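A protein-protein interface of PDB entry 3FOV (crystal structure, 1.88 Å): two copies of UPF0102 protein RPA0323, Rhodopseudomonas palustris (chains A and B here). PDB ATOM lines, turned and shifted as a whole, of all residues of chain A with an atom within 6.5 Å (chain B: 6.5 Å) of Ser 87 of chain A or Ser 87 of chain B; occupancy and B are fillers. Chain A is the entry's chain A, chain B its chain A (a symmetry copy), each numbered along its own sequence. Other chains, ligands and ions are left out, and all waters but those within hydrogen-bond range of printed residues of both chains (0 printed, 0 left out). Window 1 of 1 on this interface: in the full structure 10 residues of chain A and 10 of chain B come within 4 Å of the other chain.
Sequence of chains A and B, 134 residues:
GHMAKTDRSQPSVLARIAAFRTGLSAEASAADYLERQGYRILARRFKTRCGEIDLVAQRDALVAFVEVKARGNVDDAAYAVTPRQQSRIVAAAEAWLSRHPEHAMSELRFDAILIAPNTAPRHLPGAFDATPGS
The side-chain sulfur (SG) of Cys 50 of chain B is disulfide-bonded to the side-chain sulfur (SG) of Cys 50 of chain A (2.1 Å).
The backbone carbonyl oxygen (O) of Ser 87 of chain A is in hydrogen-bond range of the side-chain hydroxyl (OG) of Ser 87 of chain B, 2.7 Å away.
Ser 87 of chain A touches Val 90 of chain B.
Ala 91 of chain B touches Ser 87 of chain A.
CG1 of Val 90 of chain A touches CB of Ser 87 of chain B, 3.9 Å away.
OG of Ser 87 of chain B touches N of Ala 91 of chain A, at 3.9 Å.
Printed residues of chain B within 4 Å of Ser 87 of chain A: Ser 87 (2.7 Å), Val 90 (3.9 Å) and Ala 91 (3.9 Å).
Printed residues of chain A within 4 Å of Ser 87 of chain B: Ser 87 (2.7 Å), Val 90 (3.9 Å) and Ala 91 (3.9 Å).
Printed residues of chain B within 4 Å of Ala 91 of chain A: Ser 87 (3.9 Å).
Of the printed residues of chain A, Ala 91 of chain B touches Ser 87 (3.9 Å).
Printed residues of chain B within 4 Å of Val 90 of chain A: Ser 87 (3.9 Å).
Of the printed residues of chain B, Cys 50 of chain A touches Cys 50.
The nearest printed residue of chain B that does not touch Ser 87 of chain A is Arg 88 of chain B (4.8 Å).
The nearest printed residue of chain A that does not touch Ser 87 of chain B is Arg 88 of chain A (4.8 Å).
The nearest printed residue of chain B that does not touch Ala 91 of chain A is Cys 50 of chain B (6.0 Å).
Of the 14 printed residues of chain A, 4 touch a printed residue of chain B.
Hydrophobic or aromatic side chains of chain A within 4 Å of the printed part of chain B: Val 90 and Ala 91.
Hydrophobic or aromatic side chains of chain B within 4 Å of the printed part of chain A: Val 90 and Ala 91.
Among the printed residues, 6 pairs touch across the chains.
Among the printed residues, no Asp or Glu carboxylate lies within 4 Å of a Lys or Arg side-chain nitrogen of the other chain.
Cys 50 of chain B touches its own counterpart, Cys 50 of chain A.
Ser 87 of chain B touches its own counterpart, Ser 87 of chain A.
Ser 87 of chain A touches Val 90 of chain B, and with the chains exchanged Val 90 of chain A touches Ser 87 of chain B.
Ser 87 of chain A touches Ala 91 of chain B, and with the chains exchanged Ala 91 of chain A touches Ser 87 of chain B.
Of the 6 pairs that touch across the chains among the printed residues, 6 have their exchanged pair printed and touching as well.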
ATOM      1  N   CYS A  50      32.842  13.304  10.320  1.00  0.00           N
ATOM      2  CA  CYS A  50      32.118  14.521  10.673  1.00  0.00           C
ATOM      3  C   CYS A  50      32.895  15.677  11.342  1.00  0.00           C
ATOM      4  O   CYS A  50      32.306  16.730  11.706  1.00  0.00           O
ATOM      5  CB  CYS A  50      30.861  14.107  11.461  1.00  0.00           C
ATOM      6  SG  CYS A  50      29.749  13.083  10.443  1.00  0.00           S
ATOM      7  N   GLY A  51      34.207  15.531  11.429  1.00  0.00           N
ATOM      8  CA  GLY A  51      35.009  16.579  12.048  1.00  0.00           C
ATOM      9  C   GLY A  51      36.462  16.249  12.133  1.00  0.00           C
ATOM     10  O   GLY A  51      36.927  15.240  11.582  1.00  0.00           O
ATOM     11  N   THR A  82      34.152  29.353  16.249  1.00  0.00           N
ATOM     12  CA  THR A  82      32.986  29.487  15.390  1.00  0.00           C
ATOM     13  C   THR A  82      32.051  28.343  15.689  1.00  0.00           C
ATOM     14  O   THR A  82      32.510  27.261  16.020  1.00  0.00           O
ATOM     15  CB  THR A  82      33.407  29.450  13.910  1.00  0.00           C
ATOM     16  OG1 THR A  82      33.965  28.176  13.578  1.00  0.00           O
ATOM     17  CG2 THR A  82      34.470  30.519  13.632  1.00  0.00           C
ATOM     18  N   PRO A  83      30.739  28.588  15.640  1.00  0.00           N
ATOM     19  CA  PRO A  83      29.793  27.488  15.793  1.00  0.00           C
ATOM     20  C   PRO A  83      30.090  26.290  14.868  1.00  0.00           C
ATOM     21  O   PRO A  83      29.953  25.154  15.307  1.00  0.00           O
ATOM     22  CB  PRO A  83      28.458  28.147  15.477  1.00  0.00           C
ATOM     23  CG  PRO A  83      28.650  29.540  16.091  1.00  0.00           C
ATOM     24  CD  PRO A  83      30.075  29.904  15.747  1.00  0.00           C
ATOM     25  N   ARG A  84      30.529  26.551  13.629  1.00  0.00           N
ATOM     26  CA  ARG A  84      30.945  25.461  12.729  1.00  0.00           C
ATOM     27  C   ARG A  84      32.120  24.676  13.296  1.00  0.00           C
ATOM     28  O   ARG A  84      32.098  23.450  13.297  1.00  0.00           O
ATOM     29  CB  ARG A  84      31.309  25.943  11.328  1.00  0.00           C
ATOM     30  CG  ARG A  84      31.978  24.840  10.507  1.00  0.00           C
ATOM     31  CD  ARG A  84      32.003  25.128   9.041  1.00  0.00           C
ATOM     32  NE  ARG A  84      32.193  23.922   8.256  1.00  0.00           N
ATOM     33  CZ  ARG A  84      33.362  23.351   7.964  1.00  0.00           C
ATOM     34  NH1 ARG A  84      34.509  23.830   8.426  1.00  0.00           N
ATOM     35  NH2 ARG A  84      33.376  22.259   7.209  1.00  0.00           N
ATOM     36  N   GLN A  85      33.171  25.370  13.733  1.00  0.00           N
ATOM     37  CA  GLN A  85      34.320  24.627  14.234  1.00  0.00           C
ATOM     38  C   GLN A  85      33.945  23.861  15.491  1.00  0.00           C
ATOM     39  O   GLN A  85      34.403  22.773  15.654  1.00  0.00           O
ATOM     40  CB  GLN A  85      35.553  25.517  14.486  1.00  0.00           C
ATOM     41  CG  GLN A  85      36.677  25.224  13.450  1.00  0.00           C
ATOM     42  CD  GLN A  85      36.870  23.711  13.124  1.00  0.00           C
ATOM     43  OE1 GLN A  85      37.313  22.910  13.975  1.00  0.00           O
ATOM     44  NE2 GLN A  85      36.517  23.317  11.873  1.00  0.00           N
ATOM     45  N   GLN A  86      33.146  24.484  16.378  1.00  0.00           N
ATOM     46  CA  GLN A  86      32.681  23.824  17.582  1.00  0.00           C
ATOM     47  C   GLN A  86      31.931  22.544  17.224  1.00  0.00           C
ATOM     48  O   GLN A  86      32.188  21.484  17.805  1.00  0.00           O
ATOM     49  CB  GLN A  86      31.800  24.768  18.413  1.00  0.00           C
ATOM     50  CG  GLN A  86      32.597  25.929  19.018  1.00  0.00           C
ATOM     51  CD  GLN A  86      31.829  26.748  20.041  1.00  0.00           C
ATOM     52  OE1 GLN A  86      31.097  26.212  20.869  1.00  0.00           O
ATOM     53  NE2 GLN A  86      32.060  28.045  20.036  1.00  0.00           N
ATOM     54  N   SER A  87      31.031  22.640  16.256  1.00  0.00           N
ATOM     55  CA  SER A  87      30.244  21.483  15.794  1.00  0.00           C
ATOM     56  C   SER A  87      31.144  20.347  15.332  1.00  0.00           C
ATOM     57  O   SER A  87      30.901  19.155  15.652  1.00  0.00           O
ATOM     58  CB  SER A  87      29.299  21.881  14.642  1.00  0.00           C
ATOM     59  OG  SER A  87      28.788  20.733  13.950  1.00  0.00           O
ATOM     60  N   ARG A  88      32.175  20.713  14.573  1.00  0.00           N
ATOM     61  CA  ARG A  88      33.103  19.737  14.030  1.00  0.00           C
ATOM     62  C   ARG A  88      34.050  19.118  15.044  1.00  0.00           C
ATOM     63  O   ARG A  88      34.322  17.907  14.969  1.00  0.00           O
ATOM     64  CB  ARG A  88      33.889  20.346  12.883  1.00  0.00           C
ATOM     65  CG  ARG A  88      32.959  20.599  11.698  1.00  0.00           C
ATOM     66  CD  ARG A  88      33.754  21.068  10.548  1.00  0.00           C
ATOM     67  NE  ARG A  88      34.480  19.945   9.981  1.00  0.00           N
ATOM     68  CZ  ARG A  88      33.983  19.067   9.125  1.00  0.00           C
ATOM     69  NH1 ARG A  88      32.707  19.146   8.667  1.00  0.00           N
ATOM     70  NH2 ARG A  88      34.782  18.099   8.696  1.00  0.00           N
ATOM     71  N   ILE A  89      34.547  19.939  15.989  1.00  0.00           N
ATOM     72  CA  ILE A  89      35.406  19.418  17.044  1.00  0.00           C
ATOM     73  C   ILE A  89      34.617  18.553  18.033  1.00  0.00           C
ATOM     74  O   ILE A  89      35.119  17.518  18.468  1.00  0.00           O
ATOM     75  CB  ILE A  89      36.158  20.460  17.818  1.00  0.00           C
ATOM     76  CG1 ILE A  89      36.965  21.382  16.903  1.00  0.00           C
ATOM     77  CG2 ILE A  89      37.204  19.737  18.712  1.00  0.00           C
ATOM     78  CD1 ILE A  89      37.134  22.849  17.430  1.00  0.00           C
ATOM     79  N   VAL A  90      33.389  18.939  18.358  1.00  0.00           N
ATOM     80  CA  VAL A  90      32.544  18.093  19.212  1.00  0.00           C
ATOM     81  C   VAL A  90      32.247  16.765  18.520  1.00  0.00           C
ATOM     82  O   VAL A  90      32.314  15.693  19.149  1.00  0.00           O
ATOM     83  CB  VAL A  90      31.271  18.848  19.593  1.00  0.00           C
ATOM     84  CG1 VAL A  90      30.230  17.962  20.261  1.00  0.00           C
ATOM     85  CG2 VAL A  90      31.646  20.065  20.497  1.00  0.00           C
ATOM     86  N   ALA A  91      31.910  16.808  17.228  1.00  0.00           N
ATOM     87  CA  ALA A  91      31.633  15.583  16.479  1.00  0.00           C
ATOM     88  C   ALA A  91      32.867  14.672  16.445  1.00  0.00           C
ATOM     89  O   ALA A  91      32.764  13.469  16.637  1.00  0.00           O
ATOM     90  CB  ALA A  91      31.135  15.888  15.066  1.00  0.00           C
ATOM     91  N   ALA A  92      34.040  15.252  16.242  1.00  0.00           N
ATOM     92  CA  ALA A  92      35.264  14.490  16.225  1.00  0.00           C
ATOM     93  C   ALA A  92      35.608  13.969  17.633  1.00  0.00           C
ATOM     94  O   ALA A  92      36.086  12.864  17.736  1.00  0.00           O
ATOM     95  CB  ALA A  92      36.422  15.305  15.653  1.00  0.00           C
ATOM     96  N   PHE A 128      35.846  26.924  24.664  1.00  0.00           N
ATOM     97  CA  PHE A 128      34.385  26.848  24.707  1.00  0.00           C
ATOM     98  C   PHE A 128      33.934  25.720  25.617  1.00  0.00           C
ATOM     99  O   PHE A 128      34.695  24.798  25.918  1.00  0.00           O
ATOM    100  CB  PHE A 128      33.744  26.715  23.298  1.00  0.00           C
ATOM    101  CG  PHE A 128      34.111  25.437  22.549  1.00  0.00           C
ATOM    102  CD1 PHE A 128      33.268  24.328  22.575  1.00  0.00           C
ATOM    103  CD2 PHE A 128      35.268  25.370  21.774  1.00  0.00           C
ATOM    104  CE1 PHE A 128      33.586  23.161  21.861  1.00  0.00           C
ATOM    105  CE2 PHE A 128      35.586  24.208  21.054  1.00  0.00           C
ATOM    106  CZ  PHE A 128      34.758  23.119  21.096  1.00  0.00           C
ATOM    107  N   CYS B  50      26.019  13.844   8.767  1.00  0.00           N
ATOM    108  CA  CYS B  50      26.509  14.352  10.045  1.00  0.00           C
ATOM    109  C   CYS B  50      25.493  14.956  11.039  1.00  0.00           C
ATOM    110  O   CYS B  50      25.872  15.448  12.136  1.00  0.00           O
ATOM    111  CB  CYS B  50      27.695  15.291   9.753  1.00  0.00           C
ATOM    112  SG  CYS B  50      29.068  14.395   8.957  1.00  0.00           S
ATOM    113  N   GLY B  51      24.215  14.849  10.713  1.00  0.00           N
ATOM    114  CA  GLY B  51      23.196  15.395  11.601  1.00  0.00           C
ATOM    115  C   GLY B  51      21.807  15.257  11.074  1.00  0.00           C
ATOM    116  O   GLY B  51      21.568  14.600  10.050  1.00  0.00           O
ATOM    117  N   THR B  82      21.656  20.256  24.074  1.00  0.00           N
ATOM    118  CA  THR B  82      22.895  19.579  24.418  1.00  0.00           C
ATOM    119  C   THR B  82      23.935  19.955  23.394  1.00  0.00           C
ATOM    120  O   THR B  82      23.594  20.168  22.240  1.00  0.00           O
ATOM    121  CB  THR B  82      22.686  18.054  24.421  1.00  0.00           C
ATOM    122  OG1 THR B  82      22.366  17.588  23.109  1.00  0.00           O
ATOM    123  CG2 THR B  82      21.530  17.678  25.354  1.00  0.00           C
ATOM    124  N   PRO B  83      25.193  20.105  23.816  1.00  0.00           N
ATOM    125  CA  PRO B  83      26.256  20.340  22.845  1.00  0.00           C
ATOM    126  C   PRO B  83      26.260  19.329  21.680  1.00  0.00           C
ATOM    127  O   PRO B  83      26.497  19.730  20.547  1.00  0.00           O
ATOM    128  CB  PRO B  83      27.514  20.248  23.697  1.00  0.00           C
ATOM    129  CG  PRO B  83      27.046  20.892  25.008  1.00  0.00           C
ATOM    130  CD  PRO B  83      25.643  20.365  25.199  1.00  0.00           C
ATOM    131  N   ARG B  84      25.959  18.052  21.960  1.00  0.00           N
ATOM    132  CA  ARG B  84      25.828  17.054  20.885  1.00  0.00           C
ATOM    133  C   ARG B  84      24.710  17.412  19.915  1.00  0.00           C
ATOM    134  O   ARG B  84      24.906  17.359  18.705  1.00  0.00           O
ATOM    135  CB  ARG B  84      25.589  15.639  21.405  1.00  0.00           C
ATOM    136  CG  ARG B  84      25.201  14.682  20.278  1.00  0.00           C
ATOM    137  CD  ARG B  84      25.333  13.241  20.655  1.00  0.00           C
ATOM    138  NE  ARG B  84      25.423  12.382  19.487  1.00  0.00           N
ATOM    139  CZ  ARG B  84      24.398  11.901  18.785  1.00  0.00           C
ATOM    140  NH1 ARG B  84      23.142  12.218  19.075  1.00  0.00           N
ATOM    141  NH2 ARG B  84      24.640  11.103  17.753  1.00  0.00           N
ATOM    142  N   GLN B  85      23.522  17.725  20.431  1.00  0.00           N
ATOM    143  CA  GLN B  85      22.434  18.023  19.509  1.00  0.00           C
ATOM    144  C   GLN B  85      22.741  19.284  18.720  1.00  0.00           C
ATOM    145  O   GLN B  85      22.425  19.331  17.572  1.00  0.00           O
ATOM    146  CB  GLN B  85      21.064  18.139  20.207  1.00  0.00           C
ATOM    147  CG  GLN B  85      20.143  16.940  19.834  1.00  0.00           C
ATOM    148  CD  GLN B  85      20.213  16.521  18.333  1.00  0.00           C
ATOM    149  OE1 GLN B  85      19.777  17.263  17.426  1.00  0.00           O
ATOM    150  NE2 GLN B  85      20.783  15.317  18.073  1.00  0.00           N
ATOM    151  N   GLN B  86      23.317  20.304  19.385  1.00  0.00           N
ATOM    152  CA  GLN B  86      23.705  21.530  18.718  1.00  0.00           C
ATOM    153  C   GLN B  86      24.671  21.224  17.576  1.00  0.00           C
ATOM    154  O   GLN B  86      24.491  21.714  16.456  1.00  0.00           O
ATOM    155  CB  GLN B  86      24.323  22.521  19.715  1.00  0.00           C
ATOM    156  CG  GLN B  86      23.295  23.059  20.716  1.00  0.00           C
ATOM    157  CD  GLN B  86      23.794  24.217  21.563  1.00  0.00           C
ATOM    158  OE1 GLN B  86      24.477  25.115  21.077  1.00  0.00           O
ATOM    159  NE2 GLN B  86      23.384  24.239  22.815  1.00  0.00           N
ATOM    160  N   SER B  87      25.669  20.400  17.854  1.00  0.00           N
ATOM    161  CA  SER B  87      26.668  20.001  16.847  1.00  0.00           C
ATOM    162  C   SER B  87      26.009  19.365  15.632  1.00  0.00           C
ATOM    163  O   SER B  87      26.374  19.661  14.466  1.00  0.00           O
ATOM    164  CB  SER B  87      27.693  19.015  17.443  1.00  0.00           C
ATOM    165  OG  SER B  87      28.450  18.351  16.421  1.00  0.00           O
ATOM    166  N   ARG B  88      25.048  18.484  15.905  1.00  0.00           N
ATOM    167  CA  ARG B  88      24.350  17.771  14.851  1.00  0.00           C
ATOM    168  C   ARG B  88      23.373  18.610  14.046  1.00  0.00           C
ATOM    169  O   ARG B  88      23.289  18.442  12.816  1.00  0.00           O
ATOM    170  CB  ARG B  88      23.646  16.553  15.422  1.00  0.00           C
ATOM    171  CG  ARG B  88      24.682  15.525  15.875  1.00  0.00           C
ATOM    172  CD  ARG B  88      23.990  14.296  16.306  1.00  0.00           C
ATOM    173  NE  ARG B  88      23.514  13.581  15.135  1.00  0.00           N
ATOM    174  CZ  ARG B  88      24.242  12.765  14.390  1.00  0.00           C
ATOM    175  NH1 ARG B  88      25.543  12.497  14.669  1.00  0.00           N
ATOM    176  NH2 ARG B  88      23.653  12.183  13.353  1.00  0.00           N
ATOM    177  N   ILE B  89      22.642  19.511  14.728  1.00  0.00           N
ATOM    178  CA  ILE B  89      21.732  20.409  14.030  1.00  0.00           C
ATOM    179  C   ILE B  89      22.496  21.459  13.216  1.00  0.00           C
ATOM    180  O   ILE B  89      22.092  21.770  12.096  1.00  0.00           O
ATOM    181  CB  ILE B  89      20.742  21.115  14.909  1.00  0.00           C
ATOM    182  CG1 ILE B  89      19.942  20.137  15.771  1.00  0.00           C
ATOM    183  CG2 ILE B  89      19.699  21.817  13.995  1.00  0.00           C
ATOM    184  CD1 ILE B  89      19.497  20.702  17.165  1.00  0.00           C
ATOM    185  N   VAL B  90      23.601  21.973  13.741  1.00  0.00           N
ATOM    186  CA  VAL B  90      24.435  22.898  12.963  1.00  0.00           C
ATOM    187  C   VAL B  90      25.008  22.196  11.735  1.00  0.00           C
ATOM    188  O   VAL B  90      25.010  22.759  10.625  1.00  0.00           O
ATOM    189  CB  VAL B  90      25.524  23.491  13.856  1.00  0.00           C
ATOM    190  CG1 VAL B  90      26.582  24.259  13.075  1.00  0.00           C
ATOM    191  CG2 VAL B  90      24.863  24.388  14.949  1.00  0.00           C
ATOM    192  N   ALA B  91      25.506  20.968  11.907  1.00  0.00           N
ATOM    193  CA  ALA B  91      26.053  20.210  10.782  1.00  0.00           C
ATOM    194  C   ALA B  91      24.977  19.960   9.717  1.00  0.00           C
ATOM    195  O   ALA B  91      25.224  20.109   8.529  1.00  0.00           O
ATOM    196  CB  ALA B  91      26.688  18.898  11.243  1.00  0.00           C
ATOM    197  N   ALA B  92      23.772  19.619  10.146  1.00  0.00           N
ATOM    198  CA  ALA B  92      22.681  19.393   9.229  1.00  0.00           C
ATOM    199  C   ALA B  92      22.229  20.713   8.576  1.00  0.00           C
ATOM    200  O   ALA B  92      21.904  20.695   7.412  1.00  0.00           O
ATOM    201  CB  ALA B  92      21.507  18.701   9.917  1.00  0.00           C
ATOM    202  N   PHE B 128      19.208  28.225  20.895  1.00  0.00           N
ATOM    203  CA  PHE B 128      20.646  28.472  21.014  1.00  0.00           C
ATOM    204  C   PHE B 128      21.126  29.384  19.900  1.00  0.00           C
ATOM    205  O   PHE B 128      20.471  29.531  18.866  1.00  0.00           O
ATOM    206  CB  PHE B 128      21.483  27.164  21.060  1.00  0.00           C
ATOM    207  CG  PHE B 128      21.405  26.312  19.796  1.00  0.00           C
ATOM    208  CD1 PHE B 128      22.386  26.407  18.811  1.00  0.00           C
ATOM    209  CD2 PHE B 128      20.385  25.378  19.625  1.00  0.00           C
ATOM    210  CE1 PHE B 128      22.336  25.602  17.661  1.00  0.00           C
ATOM    211  CE2 PHE B 128      20.335  24.567  18.480  1.00  0.00           C
ATOM    212  CZ  PHE B 128      21.296  24.677  17.512  1.00  0.00           C
